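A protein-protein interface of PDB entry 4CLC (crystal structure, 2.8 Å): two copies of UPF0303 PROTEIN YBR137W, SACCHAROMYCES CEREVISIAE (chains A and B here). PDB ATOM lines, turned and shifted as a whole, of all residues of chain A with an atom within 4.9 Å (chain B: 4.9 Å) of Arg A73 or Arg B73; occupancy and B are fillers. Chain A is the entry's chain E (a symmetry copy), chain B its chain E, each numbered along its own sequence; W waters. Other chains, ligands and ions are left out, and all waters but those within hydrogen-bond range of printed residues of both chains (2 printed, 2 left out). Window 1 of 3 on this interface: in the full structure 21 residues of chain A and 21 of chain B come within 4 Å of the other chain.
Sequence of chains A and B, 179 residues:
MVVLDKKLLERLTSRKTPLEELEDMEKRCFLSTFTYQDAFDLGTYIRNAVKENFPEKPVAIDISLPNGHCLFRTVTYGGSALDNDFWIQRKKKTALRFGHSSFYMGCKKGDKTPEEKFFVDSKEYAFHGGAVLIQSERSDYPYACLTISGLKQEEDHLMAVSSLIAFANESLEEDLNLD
Printed residues of chain A that touch a printed residue of chain B: Cys A70, Leu A71, Phe A72, Arg A73, Thr A74, Val A75 and Asp A85.
Along chain A the printed residues that touch a printed residue of chain B span positions 70 to 85.
Printed residues of chain B that touch a printed residue of chain A: Cys B70, Leu B71, Phe B72, Arg B73, Thr B74, Val B75 and Asp B85.
Hydrophobic or aromatic side chains of chain B that line the printed part of chain A: Leu B71 and Val B75.
Among the printed residues, 13 pairs touch across the chains.
Leu A71 touches Arg B73, and with the chains exchanged Arg A73 touches Leu B71.
Leu A71 touches Val B75, and with the chains exchanged Val A75 touches Leu B71.
Phe A72 touches Arg B73, and with the chains exchanged Arg A73 touches Phe B72.
Arg A73 touches its own counterpart, Arg B73.
Of the printed residues of chain B, Leu A71 touches Arg B73, Thr B74 and Val B75.
Printed residues of chain B within 4 Å of Phe A72: Arg B73 (3.5 Å).
Of the printed residues of chain B, Arg A73 touches Cys B70, Leu B71, Phe B72 and Arg B73.
Ile B61 touches none of the printed residues of chain A.
Printed residues of chain A within 4 Å of Leu B71: Arg A73 (3.5 Å), Thr A74 (3.3 Å) and Val A75 (3.6 Å).
Arg B73 touches four residues of chain A.
Of the printed residues of chain A, Thr B74 touches Leu A71 (3.3 Å).
Of the printed residues of chain A, Val B75 touches Leu A71.
The nearest printed residue of chain A that does not touch Arg B73 is Thr A74 (5.2 Å).
Cys A70 touches Arg B73 (SG to CG, 3.7 Å).
Leu A71 touches Arg B73.
Leu A71 touches Thr B74 (O to CA, 3.3 Å).
Leu A71 touches Val B75 (O to N, 3.6 Å).
CA of Phe A72 touches O of Arg B73 (3.5 Å).
SG of Cys B70 touches CG of Arg A73, at 3.7 Å.
Arg A73 touches Leu B71.
Arg A73 touches Phe B72.
CA of Thr A74 touches O of Leu B71 (3.3 Å).
O of Leu B71 touches N of Val A75, at 3.6 Å.
The backbone NH (N) of Cys B70 lies within hydrogen-bond range of the side-chain carboxylate (OD2) of Asp A85, 2.9 Å away.
O of Arg A73 is in hydrogen-bond range of N of Arg B73 (3.2 Å).
OD2 of Asp B85 sits at hydrogen-bond distance from N of Cys A70 (2.9 Å).
Water W2 lies within hydrogen-bond range of O of Leu A71 (2.7 Å) and OG1 of Thr B74 (3.2 Å).
Water W1 lies within hydrogen-bond range of O of Leu B71 (2.7 Å) and OG1 of Thr A74 (3.2 Å).
N of Ile B61 sits at hydrogen-bond distance from O of Thr B74.
SG of Cys B70 sits at hydrogen-bond distance from OD1 of Asp B62 (3.4 Å).
OD1 of Asp B62 is in salt-bridge range of NH2 of Arg B73, at 2.7 Å.
SG of Cys B70 sits at hydrogen-bond distance from O of Phe B72 (3.7 Å).
The side-chain carboxylate of Asp A62 is in salt-bridge range of the guanidinium group of Arg A73 (2.7 Å).
The side-chain sulfur (SG) of Cys A70 is in hydrogen-bond range of the backbone carbonyl oxygen (O) of Phe A72 (3.7 Å).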
ATOM      1  N   ILE A  61      10.474 -21.125  25.282  1.00  0.00           N
ATOM      2  CA  ILE A  61      10.682 -19.688  25.449  1.00  0.00           C
ATOM      3  C   ILE A  61       9.365 -18.914  25.406  1.00  0.00           C
ATOM      4  O   ILE A  61       8.617 -19.005  24.426  1.00  0.00           O
ATOM      5  CB  ILE A  61      11.612 -19.131  24.349  1.00  0.00           C
ATOM      6  CG1 ILE A  61      12.968 -19.827  24.371  1.00  0.00           C
ATOM      7  CG2 ILE A  61      11.809 -17.647  24.493  1.00  0.00           C
ATOM      8  CD1 ILE A  61      13.811 -19.457  23.176  1.00  0.00           C
ATOM      9  N   ASP A  62       9.102 -18.130  26.450  1.00  0.00           N
ATOM     10  CA  ASP A  62       7.816 -17.440  26.596  1.00  0.00           C
ATOM     11  C   ASP A  62       7.973 -15.956  26.886  1.00  0.00           C
ATOM     12  O   ASP A  62       8.907 -15.555  27.566  1.00  0.00           O
ATOM     13  CB  ASP A  62       7.001 -18.101  27.718  1.00  0.00           C
ATOM     14  CG  ASP A  62       5.697 -17.382  28.008  1.00  0.00           C
ATOM     15  OD1 ASP A  62       4.693 -17.704  27.340  1.00  0.00           O
ATOM     16  OD2 ASP A  62       5.676 -16.514  28.917  1.00  0.00           O
ATOM     17  N   CYS A  70      -0.340 -13.993  26.786  1.00  0.00           N
ATOM     18  CA  CYS A  70       0.877 -14.518  26.179  1.00  0.00           C
ATOM     19  C   CYS A  70       1.147 -13.926  24.794  1.00  0.00           C
ATOM     20  O   CYS A  70       0.302 -14.013  23.904  1.00  0.00           O
ATOM     21  CB  CYS A  70       0.800 -16.044  26.090  1.00  0.00           C
ATOM     22  SG  CYS A  70       2.196 -16.799  25.248  1.00  0.00           S
ATOM     23  N   LEU A  71       2.282 -13.253  24.647  1.00  0.00           N
ATOM     24  CA  LEU A  71       2.697 -12.701  23.355  1.00  0.00           C
ATOM     25  C   LEU A  71       3.493 -13.698  22.503  1.00  0.00           C
ATOM     26  O   LEU A  71       3.323 -13.806  21.286  1.00  0.00           O
ATOM     27  CB  LEU A  71       3.496 -11.410  23.565  1.00  0.00           C
ATOM     28  CG  LEU A  71       2.731 -10.381  24.421  1.00  0.00           C
ATOM     29  CD1 LEU A  71       3.529  -9.115  24.629  1.00  0.00           C
ATOM     30  CD2 LEU A  71       1.373 -10.061  23.849  1.00  0.00           C
ATOM     31  N   PHE A  72       4.385 -14.428  23.143  1.00  0.00           N
ATOM     32  CA  PHE A  72       5.278 -15.273  22.390  1.00  0.00           C
ATOM     33  C   PHE A  72       5.522 -16.566  23.121  1.00  0.00           C
ATOM     34  O   PHE A  72       5.813 -16.567  24.316  1.00  0.00           O
ATOM     35  CB  PHE A  72       6.597 -14.553  22.140  1.00  0.00           C
ATOM     36  CG  PHE A  72       7.583 -15.357  21.346  1.00  0.00           C
ATOM     37  CD1 PHE A  72       7.608 -15.271  19.963  1.00  0.00           C
ATOM     38  CD2 PHE A  72       8.497 -16.183  21.980  1.00  0.00           C
ATOM     39  CE1 PHE A  72       8.516 -16.006  19.226  1.00  0.00           C
ATOM     40  CE2 PHE A  72       9.407 -16.920  21.251  1.00  0.00           C
ATOM     41  CZ  PHE A  72       9.416 -16.836  19.866  1.00  0.00           C
ATOM     42  N   ARG A  73       5.403 -17.664  22.391  1.00  0.00           N
ATOM     43  CA  ARG A  73       5.809 -18.966  22.894  1.00  0.00           C
ATOM     44  C   ARG A  73       6.488 -19.759  21.794  1.00  0.00           C
ATOM     45  O   ARG A  73       5.980 -19.807  20.672  1.00  0.00           O
ATOM     46  CB  ARG A  73       4.609 -19.744  23.414  1.00  0.00           C
ATOM     47  CG  ARG A  73       4.945 -21.146  23.824  1.00  0.00           C
ATOM     48  CD  ARG A  73       5.669 -21.118  25.132  1.00  0.00           C
ATOM     49  NE  ARG A  73       4.933 -20.334  26.117  1.00  0.00           N
ATOM     50  CZ  ARG A  73       4.137 -20.846  27.042  1.00  0.00           C
ATOM     51  NH1 ARG A  73       3.953 -22.164  27.130  1.00  0.00           N
ATOM     52  NH2 ARG A  73       3.528 -20.027  27.883  1.00  0.00           N
ATOM     53  N   THR A  74       7.626 -20.374  22.097  1.00  0.00           N
ATOM     54  CA  THR A  74       8.161 -21.391  21.203  1.00  0.00           C
ATOM     55  C   THR A  74       9.004 -22.442  21.892  1.00  0.00           C
ATOM     56  O   THR A  74       9.480 -22.255  23.018  1.00  0.00           O
ATOM     57  CB  THR A  74       9.030 -20.805  20.100  1.00  0.00           C
ATOM     58  OG1 THR A  74       9.502 -21.884  19.293  1.00  0.00           O
ATOM     59  CG2 THR A  74      10.227 -20.115  20.680  1.00  0.00           C
ATOM     60  N   VAL A  75       9.186 -23.550  21.182  1.00  0.00           N
ATOM     61  CA  VAL A  75      10.119 -24.593  21.582  1.00  0.00           C
ATOM     62  C   VAL A  75      11.246 -24.653  20.558  1.00  0.00           C
ATOM     63  O   VAL A  75      11.030 -24.409  19.370  1.00  0.00           O
ATOM     64  CB  VAL A  75       9.424 -25.965  21.722  1.00  0.00           C
ATOM     65  CG1 VAL A  75       8.473 -25.928  22.901  1.00  0.00           C
ATOM     66  CG2 VAL A  75       8.693 -26.332  20.448  1.00  0.00           C
ATOM     67  N   ASP A  85       5.667 -26.330  29.949  1.00  0.00           N
ATOM     68  CA  ASP A  85       4.575 -25.376  30.065  1.00  0.00           C
ATOM     69  C   ASP A  85       4.295 -25.063  31.524  1.00  0.00           C
ATOM     70  O   ASP A  85       4.014 -23.920  31.897  1.00  0.00           O
ATOM     71  CB  ASP A  85       3.314 -25.935  29.406  1.00  0.00           C
ATOM     72  CG  ASP A  85       3.380 -25.944  27.885  1.00  0.00           C
ATOM     73  OD1 ASP A  85       4.489 -26.035  27.325  1.00  0.00           O
ATOM     74  OD2 ASP A  85       2.311 -25.863  27.249  1.00  0.00           O
ATOM     75  N   ILE A  88       7.296 -22.943  32.898  1.00  0.00           N
ATOM     76  CA  ILE A  88       7.091 -21.567  32.460  1.00  0.00           C
ATOM     77  C   ILE A  88       6.033 -20.879  33.303  1.00  0.00           C
ATOM     78  O   ILE A  88       6.252 -19.770  33.778  1.00  0.00           O
ATOM     79  CB  ILE A  88       6.687 -21.498  30.995  1.00  0.00           C
ATOM     80  CG1 ILE A  88       7.864 -21.885  30.123  1.00  0.00           C
ATOM     81  CG2 ILE A  88       6.257 -20.101  30.617  1.00  0.00           C
ATOM     82  CD1 ILE A  88       7.474 -22.041  28.706  1.00  0.00           C
ATOM     83  N   GLN A  89       4.897 -21.546  33.517  1.00  0.00           N
ATOM     84  CA  GLN A  89       3.869 -20.990  34.394  1.00  0.00           C
ATOM     85  C   GLN A  89       4.471 -20.700  35.734  1.00  0.00           C
ATOM     86  O   GLN A  89       4.483 -19.564  36.172  1.00  0.00           O
ATOM     87  CB  GLN A  89       2.673 -21.934  34.574  1.00  0.00           C
ATOM     88  CG  GLN A  89       1.674 -21.900  33.433  1.00  0.00           C
ATOM     89  CD  GLN A  89       1.390 -20.480  32.932  1.00  0.00           C
ATOM     90  OE1 GLN A  89       1.988 -20.018  31.940  1.00  0.00           O
ATOM     91  NE2 GLN A  89       0.461 -19.787  33.604  1.00  0.00           N
ATOM     92  N   LYS A  92       7.230 -17.987  35.922  1.00  0.00           N
ATOM     93  CA  LYS A  92       6.726 -16.671  35.573  1.00  0.00           C
ATOM     94  C   LYS A  92       5.863 -16.125  36.708  1.00  0.00           C
ATOM     95  O   LYS A  92       5.893 -14.936  37.029  1.00  0.00           O
ATOM     96  CB  LYS A  92       5.954 -16.768  34.273  1.00  0.00           C
ATOM     97  CG  LYS A  92       5.199 -15.552  33.856  1.00  0.00           C
ATOM     98  CD  LYS A  92       4.447 -15.815  32.543  1.00  0.00           C
ATOM     99  CE  LYS A  92       3.358 -16.872  32.722  1.00  0.00           C
ATOM    100  NZ  LYS A  92       2.685 -17.193  31.436  1.00  0.00           N
ATOM    101  N   ILE B  61      -2.363 -16.354  17.272  1.00  0.00           N
ATOM    102  CA  ILE B  61      -2.147 -17.600  16.540  1.00  0.00           C
ATOM    103  C   ILE B  61      -1.441 -18.650  17.397  1.00  0.00           C
ATOM    104  O   ILE B  61      -0.346 -18.402  17.914  1.00  0.00           O
ATOM    105  CB  ILE B  61      -1.302 -17.359  15.270  1.00  0.00           C
ATOM    106  CG1 ILE B  61      -1.978 -16.357  14.342  1.00  0.00           C
ATOM    107  CG2 ILE B  61      -1.048 -18.639  14.524  1.00  0.00           C
ATOM    108  CD1 ILE B  61      -1.076 -15.941  13.207  1.00  0.00           C
ATOM    109  N   ASP B  62      -2.051 -19.827  17.520  1.00  0.00           N
ATOM    110  CA  ASP B  62      -1.551 -20.870  18.419  1.00  0.00           C
ATOM    111  C   ASP B  62      -1.414 -22.222  17.737  1.00  0.00           C
ATOM    112  O   ASP B  62      -2.208 -22.561  16.873  1.00  0.00           O
ATOM    113  CB  ASP B  62      -2.485 -20.997  19.632  1.00  0.00           C
ATOM    114  CG  ASP B  62      -2.098 -22.129  20.565  1.00  0.00           C
ATOM    115  OD1 ASP B  62      -1.266 -21.885  21.464  1.00  0.00           O
ATOM    116  OD2 ASP B  62      -2.641 -23.251  20.411  1.00  0.00           O
ATOM    117  N   CYS B  70       2.010 -26.387  24.364  1.00  0.00           N
ATOM    118  CA  CYS B  70       1.992 -25.322  23.368  1.00  0.00           C
ATOM    119  C   CYS B  70       3.321 -25.194  22.621  1.00  0.00           C
ATOM    120  O   CYS B  70       4.369 -25.016  23.239  1.00  0.00           O
ATOM    121  CB  CYS B  70       1.637 -23.990  24.036  1.00  0.00           C
ATOM    122  SG  CYS B  70       1.702 -22.578  22.927  1.00  0.00           S
ATOM    123  N   LEU B  71       3.281 -25.374  21.306  1.00  0.00           N
ATOM    124  CA  LEU B  71       4.467 -25.205  20.462  1.00  0.00           C
ATOM    125  C   LEU B  71       4.666 -23.760  19.986  1.00  0.00           C
ATOM    126  O   LEU B  71       5.778 -23.228  19.946  1.00  0.00           O
ATOM    127  CB  LEU B  71       4.406 -26.164  19.268  1.00  0.00           C
ATOM    128  CG  LEU B  71       4.203 -27.629  19.704  1.00  0.00           C
ATOM    129  CD1 LEU B  71       4.136 -28.565  18.520  1.00  0.00           C
ATOM    130  CD2 LEU B  71       5.259 -28.084  20.678  1.00  0.00           C
ATOM    131  N   PHE B  72       3.579 -23.118  19.607  1.00  0.00           N
ATOM    132  CA  PHE B  72       3.703 -21.814  19.003  1.00  0.00           C
ATOM    133  C   PHE B  72       2.578 -20.919  19.447  1.00  0.00           C
ATOM    134  O   PHE B  72       1.413 -21.311  19.419  1.00  0.00           O
ATOM    135  CB  PHE B  72       3.710 -21.938  17.484  1.00  0.00           C
ATOM    136  CG  PHE B  72       3.853 -20.626  16.772  1.00  0.00           C
ATOM    137  CD1 PHE B  72       5.106 -20.135  16.447  1.00  0.00           C
ATOM    138  CD2 PHE B  72       2.733 -19.892  16.410  1.00  0.00           C
ATOM    139  CE1 PHE B  72       5.245 -18.929  15.788  1.00  0.00           C
ATOM    140  CE2 PHE B  72       2.863 -18.686  15.752  1.00  0.00           C
ATOM    141  CZ  PHE B  72       4.125 -18.198  15.442  1.00  0.00           C
ATOM    142  N   ARG B  73       2.939 -19.712  19.855  1.00  0.00           N
ATOM    143  CA  ARG B  73       1.962 -18.666  20.113  1.00  0.00           C
ATOM    144  C   ARG B  73       2.484 -17.333  19.612  1.00  0.00           C
ATOM    145  O   ARG B  73       3.640 -16.993  19.867  1.00  0.00           O
ATOM    146  CB  ARG B  73       1.658 -18.566  21.600  1.00  0.00           C
ATOM    147  CG  ARG B  73       0.757 -17.418  21.944  1.00  0.00           C
ATOM    148  CD  ARG B  73      -0.644 -17.751  21.538  1.00  0.00           C
ATOM    149  NE  ARG B  73      -1.045 -19.047  22.071  1.00  0.00           N
ATOM    150  CZ  ARG B  73      -1.764 -19.217  23.170  1.00  0.00           C
ATOM    151  NH1 ARG B  73      -2.181 -18.170  23.882  1.00  0.00           N
ATOM    152  NH2 ARG B  73      -2.069 -20.448  23.547  1.00  0.00           N
ATOM    153  N   THR B  74       1.651 -16.580  18.900  1.00  0.00           N
ATOM    154  CA  THR B  74       1.967 -15.179  18.657  1.00  0.00           C
ATOM    155  C   THR B  74       0.757 -14.295  18.460  1.00  0.00           C
ATOM    156  O   THR B  74      -0.351 -14.766  18.177  1.00  0.00           O
ATOM    157  CB  THR B  74       2.844 -14.980  17.431  1.00  0.00           C
ATOM    158  OG1 THR B  74       3.085 -13.580  17.287  1.00  0.00           O
ATOM    159  CG2 THR B  74       2.140 -15.449  16.194  1.00  0.00           C
ATOM    160  N   VAL B  75       0.997 -12.996  18.607  1.00  0.00           N
ATOM    161  CA  VAL B  75       0.017 -11.975  18.269  1.00  0.00           C
ATOM    162  C   VAL B  75       0.543 -11.170  17.087  1.00  0.00           C
ATOM    163  O   VAL B  75       1.750 -10.967  16.951  1.00  0.00           O
ATOM    164  CB  VAL B  75      -0.294 -11.056  19.472  1.00  0.00           C
ATOM    165  CG1 VAL B  75      -1.024 -11.849  20.536  1.00  0.00           C
ATOM    166  CG2 VAL B  75       0.977 -10.446  20.026  1.00  0.00           C
ATOM    167  N   ASP B  85      -6.524 -15.188  24.572  1.00  0.00           N
ATOM    168  CA  ASP B  85      -5.980 -16.389  25.188  1.00  0.00           C
ATOM    169  C   ASP B  85      -7.099 -17.331  25.595  1.00  0.00           C
ATOM    170  O   ASP B  85      -6.995 -18.555  25.458  1.00  0.00           O
ATOM    171  CB  ASP B  85      -5.143 -16.021  26.413  1.00  0.00           C
ATOM    172  CG  ASP B  85      -3.808 -15.380  26.063  1.00  0.00           C
ATOM    173  OD1 ASP B  85      -3.700 -14.742  25.000  1.00  0.00           O
ATOM    174  OD2 ASP B  85      -2.863 -15.517  26.864  1.00  0.00           O
ATOM    175  N   ILE B  88      -8.677 -18.811  22.323  1.00  0.00           N
ATOM    176  CA  ILE B  88      -7.803 -19.885  21.867  1.00  0.00           C
ATOM    177  C   ILE B  88      -8.001 -21.139  22.700  1.00  0.00           C
ATOM    178  O   ILE B  88      -8.162 -22.222  22.148  1.00  0.00           O
ATOM    179  CB  ILE B  88      -6.338 -19.476  21.916  1.00  0.00           C
ATOM    180  CG1 ILE B  88      -6.063 -18.436  20.851  1.00  0.00           C
ATOM    181  CG2 ILE B  88      -5.436 -20.661  21.665  1.00  0.00           C
ATOM    182  CD1 ILE B  88      -4.714 -17.848  20.987  1.00  0.00           C
ATOM    183  N   GLN B  89      -8.019 -20.991  24.026  1.00  0.00           N
ATOM    184  CA  GLN B  89      -8.296 -22.135  24.891  1.00  0.00           C
ATOM    185  C   GLN B  89      -9.606 -22.745  24.496  1.00  0.00           C
ATOM    186  O   GLN B  89      -9.658 -23.899  24.112  1.00  0.00           O
ATOM    187  CB  GLN B  89      -8.348 -21.753  26.376  1.00  0.00           C
ATOM    188  CG  GLN B  89      -6.987 -21.625  27.035  1.00  0.00           C
ATOM    189  CD  GLN B  89      -6.017 -22.736  26.620  1.00  0.00           C
ATOM    190  OE1 GLN B  89      -5.188 -22.555  25.707  1.00  0.00           O
ATOM    191  NE2 GLN B  89      -6.104 -23.886  27.302  1.00  0.00           N
ATOM    192  N   LYS B  92      -9.864 -24.332  20.971  1.00  0.00           N
ATOM    193  CA  LYS B  92      -8.989 -25.480  20.824  1.00  0.00           C
ATOM    194  C   LYS B  92      -9.554 -26.670  21.597  1.00  0.00           C
ATOM    195  O   LYS B  92      -9.492 -27.817  21.153  1.00  0.00           O
ATOM    196  CB  LYS B  92      -7.601 -25.105  21.302  1.00  0.00           C
ATOM    197  CG  LYS B  92      -6.612 -26.216  21.407  1.00  0.00           C
ATOM    198  CD  LYS B  92      -5.268 -25.687  21.931  1.00  0.00           C
ATOM    199  CE  LYS B  92      -5.389 -25.174  23.366  1.00  0.00           C
ATOM    200  NZ  LYS B  92      -4.113 -24.582  23.847  1.00  0.00           N
HETATM  201  O   HOH W   1       6.907 -22.682  17.526  1.00  0.00           O
HETATM  202  O   HOH W   2       5.281 -12.962  19.587  1.00  0.00           O
